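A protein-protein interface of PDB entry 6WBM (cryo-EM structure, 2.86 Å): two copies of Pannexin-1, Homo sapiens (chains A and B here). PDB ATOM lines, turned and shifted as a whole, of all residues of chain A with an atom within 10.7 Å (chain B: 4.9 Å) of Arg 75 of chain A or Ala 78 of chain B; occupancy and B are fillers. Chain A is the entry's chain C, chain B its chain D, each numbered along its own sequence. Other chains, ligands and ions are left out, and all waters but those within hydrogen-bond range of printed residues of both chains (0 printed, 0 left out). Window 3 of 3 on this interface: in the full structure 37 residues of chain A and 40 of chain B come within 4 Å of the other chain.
Printed residues of chain A within 4 Å of Trp 74 of chain B: Trp 74 (3.1 Å). Ala 77 of chain B touches just one residue of chain A: Arg 75. No residue of chain A comes within 4 Å of Val 80 of chain B. Of chain A, only Arg 75 (2.5 Å) comes within 4 Å of Asp 81 of chain B. No residue of chain A comes within 4 Å of Ser 82 of chain B. Printed residues of chain B within 4 Å of Trp 74 of chain A: Trp 74.
OG of Ser 73 of chain A lies close to N of Arg 75 of chain A (3.4 Å). The side-chain hydroxyl of Ser 82 of chain B lies within hydrogen-bond range of the backbone carbonyl oxygen of Ala 78 of chain B.
Of the 10 printed residues of chain B, 4 touch a printed residue of chain A. Hydrophobic or aromatic side chains of chain B within 4 Å of the printed part of chain A: Trp 74, Ala 77 and Ala 78. Among the printed residues, Asp or Glu carboxylates within 4 Å of a Lys or Arg side-chain nitrogen of the other chain: Arg 75 of chain A with Asp 81 of chain B (2.5 Å).
Trp 74 of chain A touches its own counterpart, Trp 74 of chain B. Arg 75 of chain A touches Ala 77 of chain B, but with the chains exchanged Ala 77 of chain A does not touch Arg 75 of chain B (12.4 Å). Arg 75 of chain A touches Ala 78 of chain B, but with the chains exchanged Ala 78 of chain A does not touch Arg 75 of chain B (11.7 Å). Arg 75 of chain A touches Asp 81 of chain B, but with the chains exchanged Asp 81 of chain A does not touch Arg 75 of chain B (17.0 Å). Positions printed for both chains: 74, 75, 76, 77, 78, 79, 80, 81, 82 and 83. Of the 4 pairs that touch across the chains among the printed residues, 1 has its exchanged pair printed and touching as well.
Among the printed residues, pairs that only touch across the chains: Trp 74 of chain A with Trp 74 of chain B, Arg 75 of chain A with Ala 77 of chain B and Arg 75 of chain A with Ala 78 of chain B.
The guanidinium group (NH1) of Arg 75 of chain A lies within salt-bridge range of the side-chain carboxylate (OD2) of Asp 81 of chain B (2.5 Å).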
ATOM      1  N   CYS A  66     -37.315   8.199   6.946  1.00  0.00           N
ATOM      2  CA  CYS A  66     -36.279   9.081   7.458  1.00  0.00           C
ATOM      3  C   CYS A  66     -36.179  10.440   6.788  1.00  0.00           C
ATOM      4  O   CYS A  66     -35.468  11.301   7.314  1.00  0.00           O
ATOM      5  CB  CYS A  66     -34.914   8.392   7.378  1.00  0.00           C
ATOM      6  SG  CYS A  66     -34.670   7.173   8.683  1.00  0.00           S
ATOM      7  N   SER A  68     -34.900  11.805   3.722  1.00  0.00           N
ATOM      8  CA  SER A  68     -33.664  12.276   3.137  1.00  0.00           C
ATOM      9  C   SER A  68     -33.925  13.530   2.308  1.00  0.00           C
ATOM     10  O   SER A  68     -35.052  13.774   1.878  1.00  0.00           O
ATOM     11  CB  SER A  68     -33.062  11.186   2.264  1.00  0.00           C
ATOM     12  OG  SER A  68     -32.691  10.080   3.062  1.00  0.00           O
ATOM     13  N   PRO A  69     -32.900  14.349   2.077  1.00  0.00           N
ATOM     14  CA  PRO A  69     -33.086  15.545   1.251  1.00  0.00           C
ATOM     15  C   PRO A  69     -33.544  15.191  -0.154  1.00  0.00           C
ATOM     16  O   PRO A  69     -33.464  14.044  -0.596  1.00  0.00           O
ATOM     17  CB  PRO A  69     -31.695  16.185   1.236  1.00  0.00           C
ATOM     18  CG  PRO A  69     -31.055  15.698   2.470  1.00  0.00           C
ATOM     19  CD  PRO A  69     -31.554  14.302   2.667  1.00  0.00           C
ATOM     20  N   SER A  70     -34.035  16.209  -0.863  1.00  0.00           N
ATOM     21  CA  SER A  70     -34.548  15.994  -2.208  1.00  0.00           C
ATOM     22  C   SER A  70     -33.451  15.662  -3.206  1.00  0.00           C
ATOM     23  O   SER A  70     -33.712  14.952  -4.180  1.00  0.00           O
ATOM     24  CB  SER A  70     -35.314  17.227  -2.680  1.00  0.00           C
ATOM     25  OG  SER A  70     -35.781  17.052  -4.005  1.00  0.00           O
ATOM     26  N   SER A  71     -32.231  16.157  -2.987  1.00  0.00           N
ATOM     27  CA  SER A  71     -31.143  15.873  -3.913  1.00  0.00           C
ATOM     28  C   SER A  71     -30.763  14.400  -3.903  1.00  0.00           C
ATOM     29  O   SER A  71     -30.139  13.919  -4.854  1.00  0.00           O
ATOM     30  CB  SER A  71     -29.929  16.733  -3.573  1.00  0.00           C
ATOM     31  OG  SER A  71     -29.100  16.085  -2.626  1.00  0.00           O
ATOM     32  N   PHE A  72     -31.119  13.675  -2.849  1.00  0.00           N
ATOM     33  CA  PHE A  72     -30.799  12.260  -2.771  1.00  0.00           C
ATOM     34  C   PHE A  72     -31.540  11.480  -3.844  1.00  0.00           C
ATOM     35  O   PHE A  72     -32.646  11.842  -4.249  1.00  0.00           O
ATOM     36  CB  PHE A  72     -31.164  11.700  -1.400  1.00  0.00           C
ATOM     37  CG  PHE A  72     -30.062  11.789  -0.398  1.00  0.00           C
ATOM     38  CD1 PHE A  72     -29.106  12.777  -0.490  1.00  0.00           C
ATOM     39  CD2 PHE A  72     -29.980  10.881   0.635  1.00  0.00           C
ATOM     40  CE1 PHE A  72     -28.094  12.860   0.432  1.00  0.00           C
ATOM     41  CE2 PHE A  72     -28.972  10.959   1.559  1.00  0.00           C
ATOM     42  CZ  PHE A  72     -28.026  11.949   1.458  1.00  0.00           C
ATOM     43  N   SER A  73     -30.921  10.400  -4.307  1.00  0.00           N
ATOM     44  CA  SER A  73     -31.591   9.501  -5.226  1.00  0.00           C
ATOM     45  C   SER A  73     -32.609   8.655  -4.476  1.00  0.00           C
ATOM     46  O   SER A  73     -32.765   8.747  -3.256  1.00  0.00           O
ATOM     47  CB  SER A  73     -30.577   8.607  -5.932  1.00  0.00           C
ATOM     48  OG  SER A  73     -29.926   7.765  -4.996  1.00  0.00           O
ATOM     49  N   TRP A  74     -33.316   7.814  -5.224  1.00  0.00           N
ATOM     50  CA  TRP A  74     -34.196   6.835  -4.605  1.00  0.00           C
ATOM     51  C   TRP A  74     -33.401   5.865  -3.741  1.00  0.00           C
ATOM     52  O   TRP A  74     -33.775   5.579  -2.595  1.00  0.00           O
ATOM     53  CB  TRP A  74     -34.962   6.086  -5.691  1.00  0.00           C
ATOM     54  CG  TRP A  74     -36.056   5.227  -5.194  1.00  0.00           C
ATOM     55  CD1 TRP A  74     -37.363   5.572  -5.049  1.00  0.00           C
ATOM     56  CD2 TRP A  74     -35.954   3.862  -4.793  1.00  0.00           C
ATOM     57  NE1 TRP A  74     -38.084   4.506  -4.574  1.00  0.00           N
ATOM     58  CE2 TRP A  74     -37.238   3.443  -4.406  1.00  0.00           C
ATOM     59  CE3 TRP A  74     -34.897   2.953  -4.717  1.00  0.00           C
ATOM     60  CZ2 TRP A  74     -37.496   2.157  -3.950  1.00  0.00           C
ATOM     61  CZ3 TRP A  74     -35.155   1.677  -4.266  1.00  0.00           C
ATOM     62  CH2 TRP A  74     -36.442   1.290  -3.888  1.00  0.00           C
ATOM     63  N   ARG A  75     -32.280   5.374  -4.265  1.00  0.00           N
ATOM     64  CA  ARG A  75     -31.518   4.362  -3.550  1.00  0.00           C
ATOM     65  C   ARG A  75     -30.765   4.948  -2.367  1.00  0.00           C
ATOM     66  O   ARG A  75     -30.594   4.266  -1.355  1.00  0.00           O
ATOM     67  CB  ARG A  75     -30.558   3.665  -4.503  1.00  0.00           C
ATOM     68  CG  ARG A  75     -31.205   2.543  -5.272  1.00  0.00           C
ATOM     69  CD  ARG A  75     -31.572   1.410  -4.348  1.00  0.00           C
ATOM     70  NE  ARG A  75     -31.807   0.173  -5.081  1.00  0.00           N
ATOM     71  CZ  ARG A  75     -31.386  -1.018  -4.675  1.00  0.00           C
ATOM     72  NH1 ARG A  75     -30.708  -1.130  -3.543  1.00  0.00           N
ATOM     73  NH2 ARG A  75     -31.642  -2.096  -5.401  1.00  0.00           N
ATOM     74  N   GLN A  76     -30.309   6.196  -2.462  1.00  0.00           N
ATOM     75  CA  GLN A  76     -29.697   6.822  -1.297  1.00  0.00           C
ATOM     76  C   GLN A  76     -30.707   6.978  -0.171  1.00  0.00           C
ATOM     77  O   GLN A  76     -30.377   6.786   1.004  1.00  0.00           O
ATOM     78  CB  GLN A  76     -29.097   8.170  -1.677  1.00  0.00           C
ATOM     79  CG  GLN A  76     -28.031   8.077  -2.740  1.00  0.00           C
ATOM     80  CD  GLN A  76     -27.346   9.396  -2.989  1.00  0.00           C
ATOM     81  OE1 GLN A  76     -26.149   9.541  -2.760  1.00  0.00           O
ATOM     82  NE2 GLN A  76     -28.105  10.372  -3.458  1.00  0.00           N
ATOM     83  N   ALA A  77     -31.951   7.310  -0.514  1.00  0.00           N
ATOM     84  CA  ALA A  77     -32.996   7.389   0.497  1.00  0.00           C
ATOM     85  C   ALA A  77     -33.264   6.028   1.117  1.00  0.00           C
ATOM     86  O   ALA A  77     -33.424   5.909   2.339  1.00  0.00           O
ATOM     87  CB  ALA A  77     -34.271   7.952  -0.119  1.00  0.00           C
ATOM     88  N   ALA A  78     -33.333   4.985   0.287  1.00  0.00           N
ATOM     89  CA  ALA A  78     -33.510   3.642   0.825  1.00  0.00           C
ATOM     90  C   ALA A  78     -32.357   3.267   1.743  1.00  0.00           C
ATOM     91  O   ALA A  78     -32.558   2.623   2.781  1.00  0.00           O
ATOM     92  CB  ALA A  78     -33.642   2.635  -0.314  1.00  0.00           C
ATOM     93  N   PHE A  79     -31.138   3.665   1.378  1.00  0.00           N
ATOM     94  CA  PHE A  79     -29.987   3.391   2.226  1.00  0.00           C
ATOM     95  C   PHE A  79     -30.113   4.095   3.561  1.00  0.00           C
ATOM     96  O   PHE A  79     -29.799   3.516   4.601  1.00  0.00           O
ATOM     97  CB  PHE A  79     -28.695   3.819   1.540  1.00  0.00           C
ATOM     98  CG  PHE A  79     -27.519   3.882   2.470  1.00  0.00           C
ATOM     99  CD1 PHE A  79     -26.812   2.741   2.779  1.00  0.00           C
ATOM    100  CD2 PHE A  79     -27.129   5.076   3.040  1.00  0.00           C
ATOM    101  CE1 PHE A  79     -25.738   2.788   3.633  1.00  0.00           C
ATOM    102  CE2 PHE A  79     -26.055   5.125   3.896  1.00  0.00           C
ATOM    103  CZ  PHE A  79     -25.358   3.980   4.191  1.00  0.00           C
ATOM    104  N   VAL A  80     -30.529   5.359   3.550  1.00  0.00           N
ATOM    105  CA  VAL A  80     -30.694   6.091   4.803  1.00  0.00           C
ATOM    106  C   VAL A  80     -31.715   5.391   5.685  1.00  0.00           C
ATOM    107  O   VAL A  80     -31.503   5.199   6.889  1.00  0.00           O
ATOM    108  CB  VAL A  80     -31.098   7.547   4.529  1.00  0.00           C
ATOM    109  CG1 VAL A  80     -31.519   8.217   5.812  1.00  0.00           C
ATOM    110  CG2 VAL A  80     -29.954   8.295   3.894  1.00  0.00           C
ATOM    111  N   ASP A  81     -32.841   4.996   5.089  1.00  0.00           N
ATOM    112  CA  ASP A  81     -33.873   4.295   5.844  1.00  0.00           C
ATOM    113  C   ASP A  81     -33.318   3.033   6.490  1.00  0.00           C
ATOM    114  O   ASP A  81     -33.453   2.830   7.704  1.00  0.00           O
ATOM    115  CB  ASP A  81     -35.046   3.951   4.933  1.00  0.00           C
ATOM    116  CG  ASP A  81     -35.972   5.119   4.717  1.00  0.00           C
ATOM    117  OD1 ASP A  81     -35.712   6.194   5.291  1.00  0.00           O
ATOM    118  OD2 ASP A  81     -36.965   4.964   3.980  1.00  0.00           O
ATOM    119  N   SER A  82     -32.690   2.171   5.690  1.00  0.00           N
ATOM    120  CA  SER A  82     -32.190   0.912   6.229  1.00  0.00           C
ATOM    121  C   SER A  82     -31.096   1.147   7.256  1.00  0.00           C
ATOM    122  O   SER A  82     -31.038   0.457   8.282  1.00  0.00           O
ATOM    123  CB  SER A  82     -31.675   0.022   5.104  1.00  0.00           C
ATOM    124  OG  SER A  82     -32.730  -0.359   4.242  1.00  0.00           O
ATOM    125  N   TYR A  83     -30.221   2.116   7.002  1.00  0.00           N
ATOM    126  CA  TYR A  83     -29.144   2.399   7.935  1.00  0.00           C
ATOM    127  C   TYR A  83     -29.698   2.799   9.286  1.00  0.00           C
ATOM    128  O   TYR A  83     -29.261   2.289  10.316  1.00  0.00           O
ATOM    129  CB  TYR A  83     -28.240   3.502   7.393  1.00  0.00           C
ATOM    130  CG  TYR A  83     -26.989   3.715   8.213  1.00  0.00           C
ATOM    131  CD1 TYR A  83     -27.045   4.277   9.480  1.00  0.00           C
ATOM    132  CD2 TYR A  83     -25.748   3.373   7.713  1.00  0.00           C
ATOM    133  CE1 TYR A  83     -25.912   4.476  10.222  1.00  0.00           C
ATOM    134  CE2 TYR A  83     -24.607   3.569   8.451  1.00  0.00           C
ATOM    135  CZ  TYR A  83     -24.695   4.121   9.704  1.00  0.00           C
ATOM    136  OH  TYR A  83     -23.555   4.319  10.443  1.00  0.00           O
ATOM    137  N   CYS A  84     -30.644   3.735   9.308  1.00  0.00           N
ATOM    138  CA  CYS A  84     -31.167   4.173  10.595  1.00  0.00           C
ATOM    139  C   CYS A  84     -31.955   3.059  11.274  1.00  0.00           C
ATOM    140  O   CYS A  84     -31.889   2.902  12.501  1.00  0.00           O
ATOM    141  CB  CYS A  84     -32.011   5.427  10.407  1.00  0.00           C
ATOM    142  SG  CYS A  84     -31.091   6.777   9.636  1.00  0.00           S
ATOM    143  N   ILE A 248     -25.903   9.210   9.307  1.00  0.00           N
ATOM    144  CA  ILE A 248     -25.029   8.286   8.565  1.00  0.00           C
ATOM    145  C   ILE A 248     -23.710   9.025   8.353  1.00  0.00           C
ATOM    146  O   ILE A 248     -23.442   9.621   7.309  1.00  0.00           O
ATOM    147  CB  ILE A 248     -25.668   7.811   7.257  1.00  0.00           C
ATOM    148  CG1 ILE A 248     -26.121   8.989   6.401  1.00  0.00           C
ATOM    149  CG2 ILE A 248     -26.886   6.994   7.542  1.00  0.00           C
ATOM    150  CD1 ILE A 248     -26.488   8.604   4.998  1.00  0.00           C
ATOM    151  N   LEU A 253     -18.092   7.952   5.037  1.00  0.00           N
ATOM    152  CA  LEU A 253     -19.050   9.040   4.913  1.00  0.00           C
ATOM    153  C   LEU A 253     -18.778  10.181   5.880  1.00  0.00           C
ATOM    154  O   LEU A 253     -19.342  11.264   5.703  1.00  0.00           O
ATOM    155  CB  LEU A 253     -20.467   8.517   5.129  1.00  0.00           C
ATOM    156  CG  LEU A 253     -20.919   7.495   4.092  1.00  0.00           C
ATOM    157  CD1 LEU A 253     -22.344   7.064   4.355  1.00  0.00           C
ATOM    158  CD2 LEU A 253     -20.782   8.085   2.709  1.00  0.00           C
ATOM    159  N   PHE A 263     -30.572  13.027   9.926  1.00  0.00           N
ATOM    160  CA  PHE A 263     -31.856  12.799   9.288  1.00  0.00           C
ATOM    161  C   PHE A 263     -32.931  12.639  10.350  1.00  0.00           C
ATOM    162  O   PHE A 263     -32.676  12.116  11.437  1.00  0.00           O
ATOM    163  CB  PHE A 263     -31.831  11.554   8.403  1.00  0.00           C
ATOM    164  CG  PHE A 263     -30.805  11.603   7.314  1.00  0.00           C
ATOM    165  CD1 PHE A 263     -29.470  11.408   7.592  1.00  0.00           C
ATOM    166  CD2 PHE A 263     -31.178  11.833   6.007  1.00  0.00           C
ATOM    167  CE1 PHE A 263     -28.529  11.451   6.596  1.00  0.00           C
ATOM    168  CE2 PHE A 263     -30.237  11.875   5.005  1.00  0.00           C
ATOM    169  CZ  PHE A 263     -28.912  11.680   5.301  1.00  0.00           C
ATOM    170  N   TRP B  74     -30.508   4.390 -10.806  1.00  0.00           N
ATOM    171  CA  TRP B  74     -31.097   3.368  -9.956  1.00  0.00           C
ATOM    172  C   TRP B  74     -30.391   2.032 -10.147  1.00  0.00           C
ATOM    173  O   TRP B  74     -30.044   1.351  -9.172  1.00  0.00           O
ATOM    174  CB  TRP B  74     -32.584   3.244 -10.275  1.00  0.00           C
ATOM    175  CG  TRP B  74     -33.351   2.409  -9.328  1.00  0.00           C
ATOM    176  CD1 TRP B  74     -34.019   2.833  -8.221  1.00  0.00           C
ATOM    177  CD2 TRP B  74     -33.557   1.000  -9.406  1.00  0.00           C
ATOM    178  NE1 TRP B  74     -34.624   1.770  -7.599  1.00  0.00           N
ATOM    179  CE2 TRP B  74     -34.352   0.631  -8.308  1.00  0.00           C
ATOM    180  CE3 TRP B  74     -33.140   0.009 -10.297  1.00  0.00           C
ATOM    181  CZ2 TRP B  74     -34.740  -0.682  -8.076  1.00  0.00           C
ATOM    182  CZ3 TRP B  74     -33.527  -1.293 -10.066  1.00  0.00           C
ATOM    183  CH2 TRP B  74     -34.318  -1.628  -8.965  1.00  0.00           C
ATOM    184  N   ARG B  75     -30.144   1.658 -11.400  1.00  0.00           N
ATOM    185  CA  ARG B  75     -29.569   0.350 -11.675  1.00  0.00           C
ATOM    186  C   ARG B  75     -28.094   0.291 -11.314  1.00  0.00           C
ATOM    187  O   ARG B  75     -27.610  -0.764 -10.901  1.00  0.00           O
ATOM    188  CB  ARG B  75     -29.778  -0.010 -13.138  1.00  0.00           C
ATOM    189  CG  ARG B  75     -31.130  -0.619 -13.407  1.00  0.00           C
ATOM    190  CD  ARG B  75     -31.240  -1.972 -12.754  1.00  0.00           C
ATOM    191  NE  ARG B  75     -32.332  -2.752 -13.318  1.00  0.00           N
ATOM    192  CZ  ARG B  75     -32.252  -4.050 -13.589  1.00  0.00           C
ATOM    193  NH1 ARG B  75     -31.128  -4.708 -13.347  1.00  0.00           N
ATOM    194  NH2 ARG B  75     -33.293  -4.688 -14.102  1.00  0.00           N
ATOM    195  N   GLN B  76     -27.362   1.396 -11.457  1.00  0.00           N
ATOM    196  CA  GLN B  76     -25.978   1.398 -10.999  1.00  0.00           C
ATOM    197  C   GLN B  76     -25.906   1.206  -9.492  1.00  0.00           C
ATOM    198  O   GLN B  76     -25.024   0.504  -8.987  1.00  0.00           O
ATOM    199  CB  GLN B  76     -25.287   2.690 -11.414  1.00  0.00           C
ATOM    200  CG  GLN B  76     -25.259   2.903 -12.907  1.00  0.00           C
ATOM    201  CD  GLN B  76     -24.440   4.105 -13.304  1.00  0.00           C
ATOM    202  OE1 GLN B  76     -23.426   3.983 -13.985  1.00  0.00           O
ATOM    203  NE2 GLN B  76     -24.872   5.278 -12.875  1.00  0.00           N
ATOM    204  N   ALA B  77     -26.838   1.812  -8.757  1.00  0.00           N
ATOM    205  CA  ALA B  77     -26.890   1.604  -7.317  1.00  0.00           C
ATOM    206  C   ALA B  77     -27.212   0.155  -6.984  1.00  0.00           C
ATOM    207  O   ALA B  77     -26.604  -0.434  -6.080  1.00  0.00           O
ATOM    208  CB  ALA B  77     -27.926   2.533  -6.697  1.00  0.00           C
ATOM    209  N   ALA B  78     -28.177  -0.432  -7.694  1.00  0.00           N
ATOM    210  CA  ALA B  78     -28.479  -1.841  -7.475  1.00  0.00           C
ATOM    211  C   ALA B  78     -27.267  -2.711  -7.771  1.00  0.00           C
ATOM    212  O   ALA B  78     -27.005  -3.693  -7.063  1.00  0.00           O
ATOM    213  CB  ALA B  78     -29.666  -2.261  -8.338  1.00  0.00           C
ATOM    214  N   PHE B  79     -26.511  -2.363  -8.811  1.00  0.00           N
ATOM    215  CA  PHE B  79     -25.305  -3.112  -9.131  1.00  0.00           C
ATOM    216  C   PHE B  79     -24.288  -3.011  -8.013  1.00  0.00           C
ATOM    217  O   PHE B  79     -23.650  -4.004  -7.663  1.00  0.00           O
ATOM    218  CB  PHE B  79     -24.686  -2.612 -10.431  1.00  0.00           C
ATOM    219  CG  PHE B  79     -23.283  -3.095 -10.648  1.00  0.00           C
ATOM    220  CD1 PHE B  79     -23.047  -4.345 -11.179  1.00  0.00           C
ATOM    221  CD2 PHE B  79     -22.202  -2.307 -10.311  1.00  0.00           C
ATOM    222  CE1 PHE B  79     -21.766  -4.797 -11.376  1.00  0.00           C
ATOM    223  CE2 PHE B  79     -20.918  -2.757 -10.506  1.00  0.00           C
ATOM    224  CZ  PHE B  79     -20.700  -4.002 -11.040  1.00  0.00           C
ATOM    225  N   VAL B  80     -24.091  -1.812  -7.469  1.00  0.00           N
ATOM    226  CA  VAL B  80     -23.141  -1.649  -6.371  1.00  0.00           C
ATOM    227  C   VAL B  80     -23.558  -2.508  -5.189  1.00  0.00           C
ATOM    228  O   VAL B  80     -22.737  -3.207  -4.580  1.00  0.00           O
ATOM    229  CB  VAL B  80     -23.027  -0.170  -5.973  1.00  0.00           C
ATOM    230  CG1 VAL B  80     -22.256  -0.040  -4.683  1.00  0.00           C
ATOM    231  CG2 VAL B  80     -22.355   0.615  -7.070  1.00  0.00           C
ATOM    232  N   ASP B  81     -24.848  -2.470  -4.853  1.00  0.00           N
ATOM    233  CA  ASP B  81     -25.350  -3.276  -3.748  1.00  0.00           C
ATOM    234  C   ASP B  81     -25.056  -4.755  -3.969  1.00  0.00           C
ATOM    235  O   ASP B  81     -24.471  -5.420  -3.106  1.00  0.00           O
ATOM    236  CB  ASP B  81     -26.849  -3.056  -3.577  1.00  0.00           C
ATOM    237  CG  ASP B  81     -27.164  -1.792  -2.821  1.00  0.00           C
ATOM    238  OD1 ASP B  81     -26.216  -1.094  -2.413  1.00  0.00           O
ATOM    239  OD2 ASP B  81     -28.360  -1.496  -2.627  1.00  0.00           O
ATOM    240  N   SER B  82     -25.458  -5.283  -5.125  1.00  0.00           N
ATOM    241  CA  SER B  82     -25.267  -6.707  -5.377  1.00  0.00           C
ATOM    242  C   SER B  82     -23.792  -7.063  -5.435  1.00  0.00           C
ATOM    243  O   SER B  82     -23.379  -8.117  -4.933  1.00  0.00           O
ATOM    244  CB  SER B  82     -25.960  -7.112  -6.673  1.00  0.00           C
ATOM    245  OG  SER B  82     -27.362  -6.962  -6.562  1.00  0.00           O
ATOM    246  N   TYR B  83     -22.981  -6.200  -6.042  1.00  0.00           N
ATOM    247  CA  TYR B  83     -21.557  -6.474  -6.140  1.00  0.00           C
ATOM    248  C   TYR B  83     -20.940  -6.598  -4.764  1.00  0.00           C
ATOM    249  O   TYR B  83     -20.197  -7.540  -4.495  1.00  0.00           O
ATOM    250  CB  TYR B  83     -20.854  -5.375  -6.931  1.00  0.00           C
ATOM    251  CG  TYR B  83     -19.409  -5.687  -7.246  1.00  0.00           C
ATOM    252  CD1 TYR B  83     -18.443  -5.695  -6.251  1.00  0.00           C
ATOM    253  CD2 TYR B  83     -19.008  -5.953  -8.539  1.00  0.00           C
ATOM    254  CE1 TYR B  83     -17.131  -5.973  -6.534  1.00  0.00           C
ATOM    255  CE2 TYR B  83     -17.695  -6.231  -8.832  1.00  0.00           C
ATOM    256  CZ  TYR B  83     -16.762  -6.239  -7.826  1.00  0.00           C
ATOM    257  OH  TYR B  83     -15.449  -6.516  -8.115  1.00  0.00           O
